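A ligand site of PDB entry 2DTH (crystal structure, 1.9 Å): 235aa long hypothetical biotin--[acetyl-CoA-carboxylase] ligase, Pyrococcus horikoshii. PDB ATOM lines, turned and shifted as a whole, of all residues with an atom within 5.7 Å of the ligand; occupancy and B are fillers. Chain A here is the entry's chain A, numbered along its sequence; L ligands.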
ATOM      1  N   THR A  20      24.484  12.874   5.654  1.00  0.00           N
ATOM      2  CA  THR A  20      24.382  12.378   7.012  1.00  0.00           C
ATOM      3  C   THR A  20      23.068  12.901   7.582  1.00  0.00           C
ATOM      4  O   THR A  20      22.219  12.126   8.029  1.00  0.00           O
ATOM      5  CB  THR A  20      25.574  12.872   7.869  1.00  0.00           C
ATOM      6  OG1 THR A  20      25.745  14.283   7.692  1.00  0.00           O
ATOM      7  CG2 THR A  20      26.855  12.141   7.467  1.00  0.00           C
ATOM      8  N   SER A  21      22.887  14.216   7.540  1.00  0.00           N
ATOM      9  CA  SER A  21      21.672  14.857   8.031  1.00  0.00           C
ATOM     10  C   SER A  21      21.551  16.234   7.406  1.00  0.00           C
ATOM     11  O   SER A  21      22.523  16.994   7.374  1.00  0.00           O
ATOM     12  CB  SER A  21      21.705  14.966   9.558  1.00  0.00           C
ATOM     13  OG  SER A  21      20.639  15.779  10.038  1.00  0.00           O
ATOM     14  N   THR A  22      20.366  16.563   6.911  1.00  0.00           N
ATOM     15  CA  THR A  22      20.161  17.858   6.295  1.00  0.00           C
ATOM     16  C   THR A  22      20.206  18.930   7.378  1.00  0.00           C
ATOM     17  O   THR A  22      20.584  20.065   7.109  1.00  0.00           O
ATOM     18  CB  THR A  22      18.805  17.939   5.540  1.00  0.00           C
ATOM     19  OG1 THR A  22      17.736  17.637   6.437  1.00  0.00           O
ATOM     20  CG2 THR A  22      18.798  16.957   4.360  1.00  0.00           C
ATOM     21  N   ASN A  23      19.804  18.581   8.605  1.00  0.00           N
ATOM     22  CA  ASN A  23      19.818  19.552   9.685  1.00  0.00           C
ATOM     23  C   ASN A  23      21.252  19.944  10.069  1.00  0.00           C
ATOM     24  O   ASN A  23      21.534  21.081  10.436  1.00  0.00           O
ATOM     25  CB  ASN A  23      19.078  19.004  10.909  1.00  0.00           C
ATOM     26  CG  ASN A  23      17.732  19.678  11.130  1.00  0.00           C
ATOM     27  OD1 ASN A  23      16.961  19.863  10.188  1.00  0.00           O
ATOM     28  ND2 ASN A  23      17.446  20.049  12.366  1.00  0.00           N
ATOM     29  N   GLN A  42      19.108   9.994   4.243  1.00  0.00           N
ATOM     30  CA  GLN A  42      19.985  10.465   5.305  1.00  0.00           C
ATOM     31  C   GLN A  42      20.527   9.216   5.994  1.00  0.00           C
ATOM     32  O   GLN A  42      19.778   8.265   6.235  1.00  0.00           O
ATOM     33  CB  GLN A  42      19.228  11.309   6.326  1.00  0.00           C
ATOM     34  CG  GLN A  42      18.789  12.655   5.799  1.00  0.00           C
ATOM     35  CD  GLN A  42      18.081  13.494   6.850  1.00  0.00           C
ATOM     36  OE1 GLN A  42      18.387  14.671   7.002  1.00  0.00           O
ATOM     37  NE2 GLN A  42      17.152  12.884   7.575  1.00  0.00           N
ATOM     38  N   MET A  44      22.252   9.516   8.898  1.00  0.00           N
ATOM     39  CA  MET A  44      22.260   9.866  10.311  1.00  0.00           C
ATOM     40  C   MET A  44      21.140  10.827  10.665  1.00  0.00           C
ATOM     41  O   MET A  44      21.351  11.805  11.369  1.00  0.00           O
ATOM     42  CB  MET A  44      23.598  10.497  10.704  1.00  0.00           C
ATOM     43  CG  MET A  44      24.785   9.564  10.632  1.00  0.00           C
ATOM     44  SD  MET A  44      24.779   8.368  11.985  1.00  0.00           S
ATOM     45  CE  MET A  44      25.230   9.448  13.365  1.00  0.00           C
ATOM     46  N   GLY A  45      19.944  10.558  10.144  1.00  0.00           N
ATOM     47  CA  GLY A  45      18.825  11.431  10.442  1.00  0.00           C
ATOM     48  C   GLY A  45      18.423  11.229  11.881  1.00  0.00           C
ATOM     49  O   GLY A  45      18.495  10.125  12.409  1.00  0.00           O
ATOM     50  N   HIS A  46      17.998  12.294  12.546  1.00  0.00           N
ATOM     51  CA  HIS A  46      17.577  12.148  13.940  1.00  0.00           C
ATOM     52  C   HIS A  46      16.406  13.037  14.299  1.00  0.00           C
ATOM     53  O   HIS A  46      16.120  13.996  13.586  1.00  0.00           O
ATOM     54  CB  HIS A  46      18.758  12.430  14.872  1.00  0.00           C
ATOM     55  CG  HIS A  46      19.361  13.781  14.666  1.00  0.00           C
ATOM     56  ND1 HIS A  46      20.421  14.003  13.801  1.00  0.00           N
ATOM     57  CD2 HIS A  46      19.099  14.972  15.242  1.00  0.00           C
ATOM     58  CE1 HIS A  46      20.773  15.273  13.859  1.00  0.00           C
ATOM     59  NE2 HIS A  46      19.985  15.880  14.726  1.00  0.00           N
ATOM     60  N   GLY A  47      15.736  12.719  15.409  1.00  0.00           N
ATOM     61  CA  GLY A  47      14.592  13.504  15.825  1.00  0.00           C
ATOM     62  C   GLY A  47      14.814  14.375  17.045  1.00  0.00           C
ATOM     63  O   GLY A  47      15.948  14.573  17.494  1.00  0.00           O
ATOM     64  N   ARG A  48      13.678  14.834  17.577  1.00  0.00           N
ATOM     65  CA  ARG A  48      13.513  15.723  18.729  1.00  0.00           C
ATOM     66  C   ARG A  48      14.306  15.340  19.964  1.00  0.00           C
ATOM     67  O   ARG A  48      15.047  16.160  20.525  1.00  0.00           O
ATOM     68  CB  ARG A  48      12.018  15.758  19.096  1.00  0.00           C
ATOM     69  CG  ARG A  48      11.597  16.956  19.906  1.00  0.00           C
ATOM     70  CD  ARG A  48      10.089  17.100  19.883  1.00  0.00           C
ATOM     71  NE  ARG A  48       9.568  16.687  21.168  1.00  0.00           N
ATOM     72  CZ  ARG A  48       8.659  15.744  21.372  1.00  0.00           C
ATOM     73  NH1 ARG A  48       8.111  15.050  20.365  1.00  0.00           N
ATOM     74  NH2 ARG A  48       8.294  15.494  22.617  1.00  0.00           N
ATOM     75  N   LEU A  49      14.103  14.108  20.410  1.00  0.00           N
ATOM     76  CA  LEU A  49      14.795  13.645  21.587  1.00  0.00           C
ATOM     77  C   LEU A  49      16.102  12.967  21.273  1.00  0.00           C
ATOM     78  O   LEU A  49      16.629  12.222  22.093  1.00  0.00           O
ATOM     79  CB  LEU A  49      13.923  12.715  22.396  1.00  0.00           C
ATOM     80  CG  LEU A  49      12.681  13.389  23.030  1.00  0.00           C
ATOM     81  CD1 LEU A  49      11.835  12.302  23.660  1.00  0.00           C
ATOM     82  CD2 LEU A  49      13.108  14.436  24.073  1.00  0.00           C
ATOM     83  N   TRP A  53      16.020   8.949  13.111  1.00  0.00           N
ATOM     84  CA  TRP A  53      14.882   9.161  12.228  1.00  0.00           C
ATOM     85  C   TRP A  53      15.194   8.413  10.952  1.00  0.00           C
ATOM     86  O   TRP A  53      16.106   8.795  10.208  1.00  0.00           O
ATOM     87  CB  TRP A  53      14.670  10.643  11.942  1.00  0.00           C
ATOM     88  CG  TRP A  53      13.535  10.896  10.984  1.00  0.00           C
ATOM     89  CD1 TRP A  53      13.634  11.129   9.644  1.00  0.00           C
ATOM     90  CD2 TRP A  53      12.137  10.921  11.293  1.00  0.00           C
ATOM     91  NE1 TRP A  53      12.384  11.304   9.100  1.00  0.00           N
ATOM     92  CE2 TRP A  53      11.448  11.181  10.081  1.00  0.00           C
ATOM     93  CE3 TRP A  53      11.394  10.762  12.475  1.00  0.00           C
ATOM     94  CZ2 TRP A  53      10.056  11.276  10.029  1.00  0.00           C
ATOM     95  CZ3 TRP A  53      10.012  10.854  12.406  1.00  0.00           C
ATOM     96  CH2 TRP A  53       9.352  11.111  11.189  1.00  0.00           C
ATOM     97  N   SER A  55      15.405   7.515   7.412  1.00  0.00           N
ATOM     98  CA  SER A  55      15.311   8.354   6.222  1.00  0.00           C
ATOM     99  C   SER A  55      15.661   7.631   4.917  1.00  0.00           C
ATOM    100  O   SER A  55      16.622   8.000   4.240  1.00  0.00           O
ATOM    101  CB  SER A  55      16.243   9.556   6.388  1.00  0.00           C
ATOM    102  OG  SER A  55      16.044  10.196   7.631  1.00  0.00           O
ATOM    103  N   LEU A  60      10.489  12.667   2.164  1.00  0.00           N
ATOM    104  CA  LEU A  60      10.968  14.024   2.001  1.00  0.00           C
ATOM    105  C   LEU A  60      11.705  14.422   3.274  1.00  0.00           C
ATOM    106  O   LEU A  60      11.100  14.581   4.333  1.00  0.00           O
ATOM    107  CB  LEU A  60       9.808  14.995   1.755  1.00  0.00           C
ATOM    108  CG  LEU A  60      10.248  16.355   1.217  1.00  0.00           C
ATOM    109  CD1 LEU A  60      10.924  16.165  -0.147  1.00  0.00           C
ATOM    110  CD2 LEU A  60       9.032  17.279   1.110  1.00  0.00           C
ATOM    111  N   TRP A  61      13.011  14.565   3.142  1.00  0.00           N
ATOM    112  CA  TRP A  61      13.870  14.927   4.258  1.00  0.00           C
ATOM    113  C   TRP A  61      14.502  16.267   3.907  1.00  0.00           C
ATOM    114  O   TRP A  61      15.346  16.344   3.009  1.00  0.00           O
ATOM    115  CB  TRP A  61      14.936  13.844   4.443  1.00  0.00           C
ATOM    116  CG  TRP A  61      14.446  12.435   4.116  1.00  0.00           C
ATOM    117  CD1 TRP A  61      14.983  11.577   3.177  1.00  0.00           C
ATOM    118  CD2 TRP A  61      13.363  11.729   4.730  1.00  0.00           C
ATOM    119  NE1 TRP A  61      14.287  10.385   3.174  1.00  0.00           N
ATOM    120  CE2 TRP A  61      13.290  10.453   4.122  1.00  0.00           C
ATOM    121  CE3 TRP A  61      12.434  12.056   5.734  1.00  0.00           C
ATOM    122  CZ2 TRP A  61      12.324   9.493   4.483  1.00  0.00           C
ATOM    123  CZ3 TRP A  61      11.476  11.100   6.100  1.00  0.00           C
ATOM    124  CH2 TRP A  61      11.431   9.837   5.471  1.00  0.00           C
ATOM    125  N   LEU A  62      14.093  17.341   4.580  1.00  0.00           N
ATOM    126  CA  LEU A  62      14.639  18.658   4.276  1.00  0.00           C
ATOM    127  C   LEU A  62      14.848  19.525   5.500  1.00  0.00           C
ATOM    128  O   LEU A  62      14.315  19.256   6.579  1.00  0.00           O
ATOM    129  CB  LEU A  62      13.720  19.391   3.285  1.00  0.00           C
ATOM    130  CG  LEU A  62      12.258  19.646   3.670  1.00  0.00           C
ATOM    131  CD1 LEU A  62      12.157  20.832   4.624  1.00  0.00           C
ATOM    132  CD2 LEU A  62      11.435  19.920   2.412  1.00  0.00           C
ATOM    133  N   SER A  63      15.639  20.579   5.313  1.00  0.00           N
ATOM    134  CA  SER A  63      15.934  21.530   6.376  1.00  0.00           C
ATOM    135  C   SER A  63      15.947  22.916   5.769  1.00  0.00           C
ATOM    136  O   SER A  63      16.410  23.108   4.639  1.00  0.00           O
ATOM    137  CB  SER A  63      17.292  21.227   7.016  1.00  0.00           C
ATOM    138  OG  SER A  63      17.248  19.989   7.721  1.00  0.00           O
ATOM    139  N   ASN A 103       5.596  18.872  17.984  1.00  0.00           N
ATOM    140  CA  ASN A 103       6.109  18.810  16.608  1.00  0.00           C
ATOM    141  C   ASN A 103       5.677  17.675  15.695  1.00  0.00           C
ATOM    142  O   ASN A 103       6.041  17.657  14.517  1.00  0.00           O
ATOM    143  CB  ASN A 103       7.632  18.763  16.694  1.00  0.00           C
ATOM    144  CG  ASN A 103       8.139  17.443  17.256  1.00  0.00           C
ATOM    145  OD1 ASN A 103       7.617  16.962  18.270  1.00  0.00           O
ATOM    146  ND2 ASN A 103       9.136  16.860  16.616  1.00  0.00           N
ATOM    147  N   ASP A 104       4.940  16.705  16.204  1.00  0.00           N
ATOM    148  CA  ASP A 104       4.552  15.572  15.375  1.00  0.00           C
ATOM    149  C   ASP A 104       3.244  15.735  14.611  1.00  0.00           C
ATOM    150  O   ASP A 104       2.359  16.485  15.021  1.00  0.00           O
ATOM    151  CB  ASP A 104       4.467  14.297  16.226  1.00  0.00           C
ATOM    152  CG  ASP A 104       5.742  14.025  17.000  1.00  0.00           C
ATOM    153  OD1 ASP A 104       6.851  14.137  16.429  1.00  0.00           O
ATOM    154  OD2 ASP A 104       5.633  13.691  18.198  1.00  0.00           O
ATOM    155  N   LYS A 111       2.278   8.187  13.110  1.00  0.00           N
ATOM    156  CA  LYS A 111       3.205   9.262  12.730  1.00  0.00           C
ATOM    157  C   LYS A 111       3.598   9.264  11.249  1.00  0.00           C
ATOM    158  O   LYS A 111       4.192   8.310  10.748  1.00  0.00           O
ATOM    159  CB  LYS A 111       4.455   9.204  13.618  1.00  0.00           C
ATOM    160  CG  LYS A 111       5.377  10.432  13.504  1.00  0.00           C
ATOM    161  CD  LYS A 111       6.495  10.370  14.537  1.00  0.00           C
ATOM    162  CE  LYS A 111       7.283  11.682  14.623  1.00  0.00           C
ATOM    163  NZ  LYS A 111       8.288  11.651  15.726  1.00  0.00           N
ATOM    164  N   ALA A 113       4.949  12.351   9.981  1.00  0.00           N
ATOM    165  CA  ALA A 113       5.987  13.369   9.887  1.00  0.00           C
ATOM    166  C   ALA A 113       6.470  13.848  11.255  1.00  0.00           C
ATOM    167  O   ALA A 113       5.772  13.728  12.258  1.00  0.00           O
ATOM    168  CB  ALA A 113       5.485  14.550   9.068  1.00  0.00           C
ATOM    169  N   GLY A 114       7.691  14.371  11.256  1.00  0.00           N
ATOM    170  CA  GLY A 114       8.289  14.891  12.474  1.00  0.00           C
ATOM    171  C   GLY A 114       9.003  16.186  12.132  1.00  0.00           C
ATOM    172  O   GLY A 114       9.511  16.330  11.013  1.00  0.00           O
ATOM    173  N   VAL A 115       9.051  17.106  13.077  1.00  0.00           N
ATOM    174  CA  VAL A 115       9.682  18.415  12.883  1.00  0.00           C
ATOM    175  C   VAL A 115      10.757  18.617  13.942  1.00  0.00           C
ATOM    176  O   VAL A 115      10.513  18.424  15.131  1.00  0.00           O
ATOM    177  CB  VAL A 115       8.641  19.570  13.017  1.00  0.00           C
ATOM    178  CG1 VAL A 115       9.328  20.927  12.837  1.00  0.00           C
ATOM    179  CG2 VAL A 115       7.524  19.398  11.987  1.00  0.00           C
ATOM    180  N   LEU A 116      11.954  19.013  13.505  1.00  0.00           N
ATOM    181  CA  LEU A 116      13.065  19.240  14.416  1.00  0.00           C
ATOM    182  C   LEU A 116      13.671  20.621  14.196  1.00  0.00           C
ATOM    183  O   LEU A 116      14.322  20.866  13.179  1.00  0.00           O
ATOM    184  CB  LEU A 116      14.155  18.183  14.225  1.00  0.00           C
ATOM    185  CG  LEU A 116      15.431  18.392  15.049  1.00  0.00           C
ATOM    186  CD1 LEU A 116      15.126  18.175  16.535  1.00  0.00           C
ATOM    187  CD2 LEU A 116      16.487  17.430  14.576  1.00  0.00           C
ATOM    188  N   GLY A 127      13.908  21.608  10.527  1.00  0.00           N
ATOM    189  CA  GLY A 127      13.971  20.331   9.847  1.00  0.00           C
ATOM    190  C   GLY A 127      12.631  19.606   9.808  1.00  0.00           C
ATOM    191  O   GLY A 127      11.899  19.581  10.799  1.00  0.00           O
ATOM    192  N   ILE A 128      12.324  19.011   8.657  1.00  0.00           N
ATOM    193  CA  ILE A 128      11.076  18.274   8.498  1.00  0.00           C
ATOM    194  C   ILE A 128      11.305  16.938   7.774  1.00  0.00           C
ATOM    195  O   ILE A 128      12.032  16.867   6.772  1.00  0.00           O
ATOM    196  CB  ILE A 128      10.035  19.081   7.670  1.00  0.00           C
ATOM    197  CG1 ILE A 128       9.764  20.428   8.344  1.00  0.00           C
ATOM    198  CG2 ILE A 128       8.728  18.281   7.521  1.00  0.00           C
ATOM    199  CD1 ILE A 128       8.957  21.407   7.484  1.00  0.00           C
ATOM    200  N   GLY A 129      10.698  15.894   8.325  1.00  0.00           N
ATOM    201  CA  GLY A 129      10.772  14.563   7.731  1.00  0.00           C
ATOM    202  C   GLY A 129       9.334  14.159   7.441  1.00  0.00           C
ATOM    203  O   GLY A 129       8.531  14.059   8.356  1.00  0.00           O
HETATM  204  C1  LIG L   1      10.905  14.160  15.358  1.00  0.00           C
HETATM  205  O1  LIG L   1      11.266  14.037  16.554  1.00  0.00           O
HETATM  206  O2  LIG L   1       9.906  13.529  14.884  1.00  0.00           O
HETATM  207  C2  LIG L   1      11.653  15.044  14.424  1.00  0.00           C
HETATM  208  C3  LIG L   1      12.097  14.368  13.155  1.00  0.00           C
HETATM  209  C4  LIG L   1      12.753  15.324  12.201  1.00  0.00           C
HETATM  210  C5  LIG L   1      13.213  14.642  10.931  1.00  0.00           C
HETATM  211  C6  LIG L   1      13.900  15.560   9.907  1.00  0.00           C
HETATM  212  S1  LIG L   1      14.442  14.698   8.469  1.00  0.00           S
HETATM  213  C7  LIG L   1      15.154  16.242   7.862  1.00  0.00           C
HETATM  214  C8  LIG L   1      15.945  16.713   9.096  1.00  0.00           C
HETATM  215  N1  LIG L   1      17.252  16.050   9.214  1.00  0.00           N
HETATM  216  C9  LIG L   1      17.311  15.347  10.349  1.00  0.00           C
HETATM  217  O3  LIG L   1      18.303  14.666  10.718  1.00  0.00           O
HETATM  218  N2  LIG L   1      16.150  15.465  11.075  1.00  0.00           N
HETATM  219  C10 LIG L   1      15.198  16.315  10.397  1.00  0.00           C
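O2 of the ligand lies within salt-bridge range of NZ of Lys 111.
The side-chain hydroxyl of Ser 21 sits at hydrogen-bond distance from an oxygen (O3) of the ligand (2.7 Å).
An oxygen (O1) of the ligand is in hydrogen-bond range of the backbone NH (N) of Arg 48 (2.7 Å).
N1 of the ligand is in hydrogen-bond range of OE1 of Gln 42, 2.8 Å away.
O3 of the ligand sits at hydrogen-bond distance from N of His 46, at 3.0 Å.
A nitrogen (N2) of the ligand sits at hydrogen-bond distance from the backbone carbonyl oxygen of His 46, at 2.9 Å.
OG1 of Thr 22 sits at hydrogen-bond distance from N1 of the ligand (3.2 Å).
The side-chain amino group of Lys 111 lies within salt-bridge range of the side-chain carboxylate of Asp 104, at 3.0 Å.
NH1 of Arg 48 is in salt-bridge range of OD2 of Asp 104, 3.6 Å away.
The side-chain hydroxyl (OG1) of Thr 22 sits at hydrogen-bond distance from the side-chain hydroxyl (OG) of Ser 63.
O of Gly 45 sits at hydrogen-bond distance from N of Trp 53, 2.8 Å away.
O of Thr 20 lies within hydrogen-bond range of N of Gly 45 (3.5 Å).
The side-chain carboxylate (OD1) of Asp 104 sits close to the side-chain amide oxygen (OD1) of Asn 103, 3.5 Å away.
The side-chain amide nitrogen (ND2) of Asn 103 is in hydrogen-bond range of the backbone carbonyl oxygen (O) of Val 115.
The backbone carbonyl oxygen (O) of Leu 116 sits at hydrogen-bond distance from the side-chain amide nitrogen (ND2) of Asn 23 (3.3 Å).
O2 of the ligand sits close to OD1 of Asp 104 (3.5 Å).
O of Ile 128 sits close to S1 of the ligand.
OD1 of Asn 23 touches C8 of the ligand, at 3.5 Å.
Gly 45 touches the ligand (CA to O3, 3.3 Å).
CA of Gly 47 touches O1 of the ligand, 3.4 Å away.
Trp 53 touches the ligand (CZ3 to O2, 3.6 Å).
O of Leu 62 touches C7 of the ligand (3.4 Å).
OG of Ser 63 touches C8 of the ligand (3.8 Å).
Asn 103 touches the ligand.
CA of Gly 114 touches O2 of the ligand (3.2 Å).
Val 115 touches the ligand.
Leu 116 touches the ligand (CB to C4, 3.8 Å).
Gly 129 touches the ligand (N to C6, 3.6 Å).
Within 4 Å of the ligand: Ser 21, Thr 22, Asn 23, Gln 42, Gly 45, His 46, Gly 47, Arg 48, Trp 53, Leu 62, Ser 63, Asn 103, Asp 104, Lys 111, Gly 114, Val 115, Leu 116, Ile 128 and Gly 129.
The nearest printed residue that does not touch the ligand is Trp 61 (4.01 Å).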
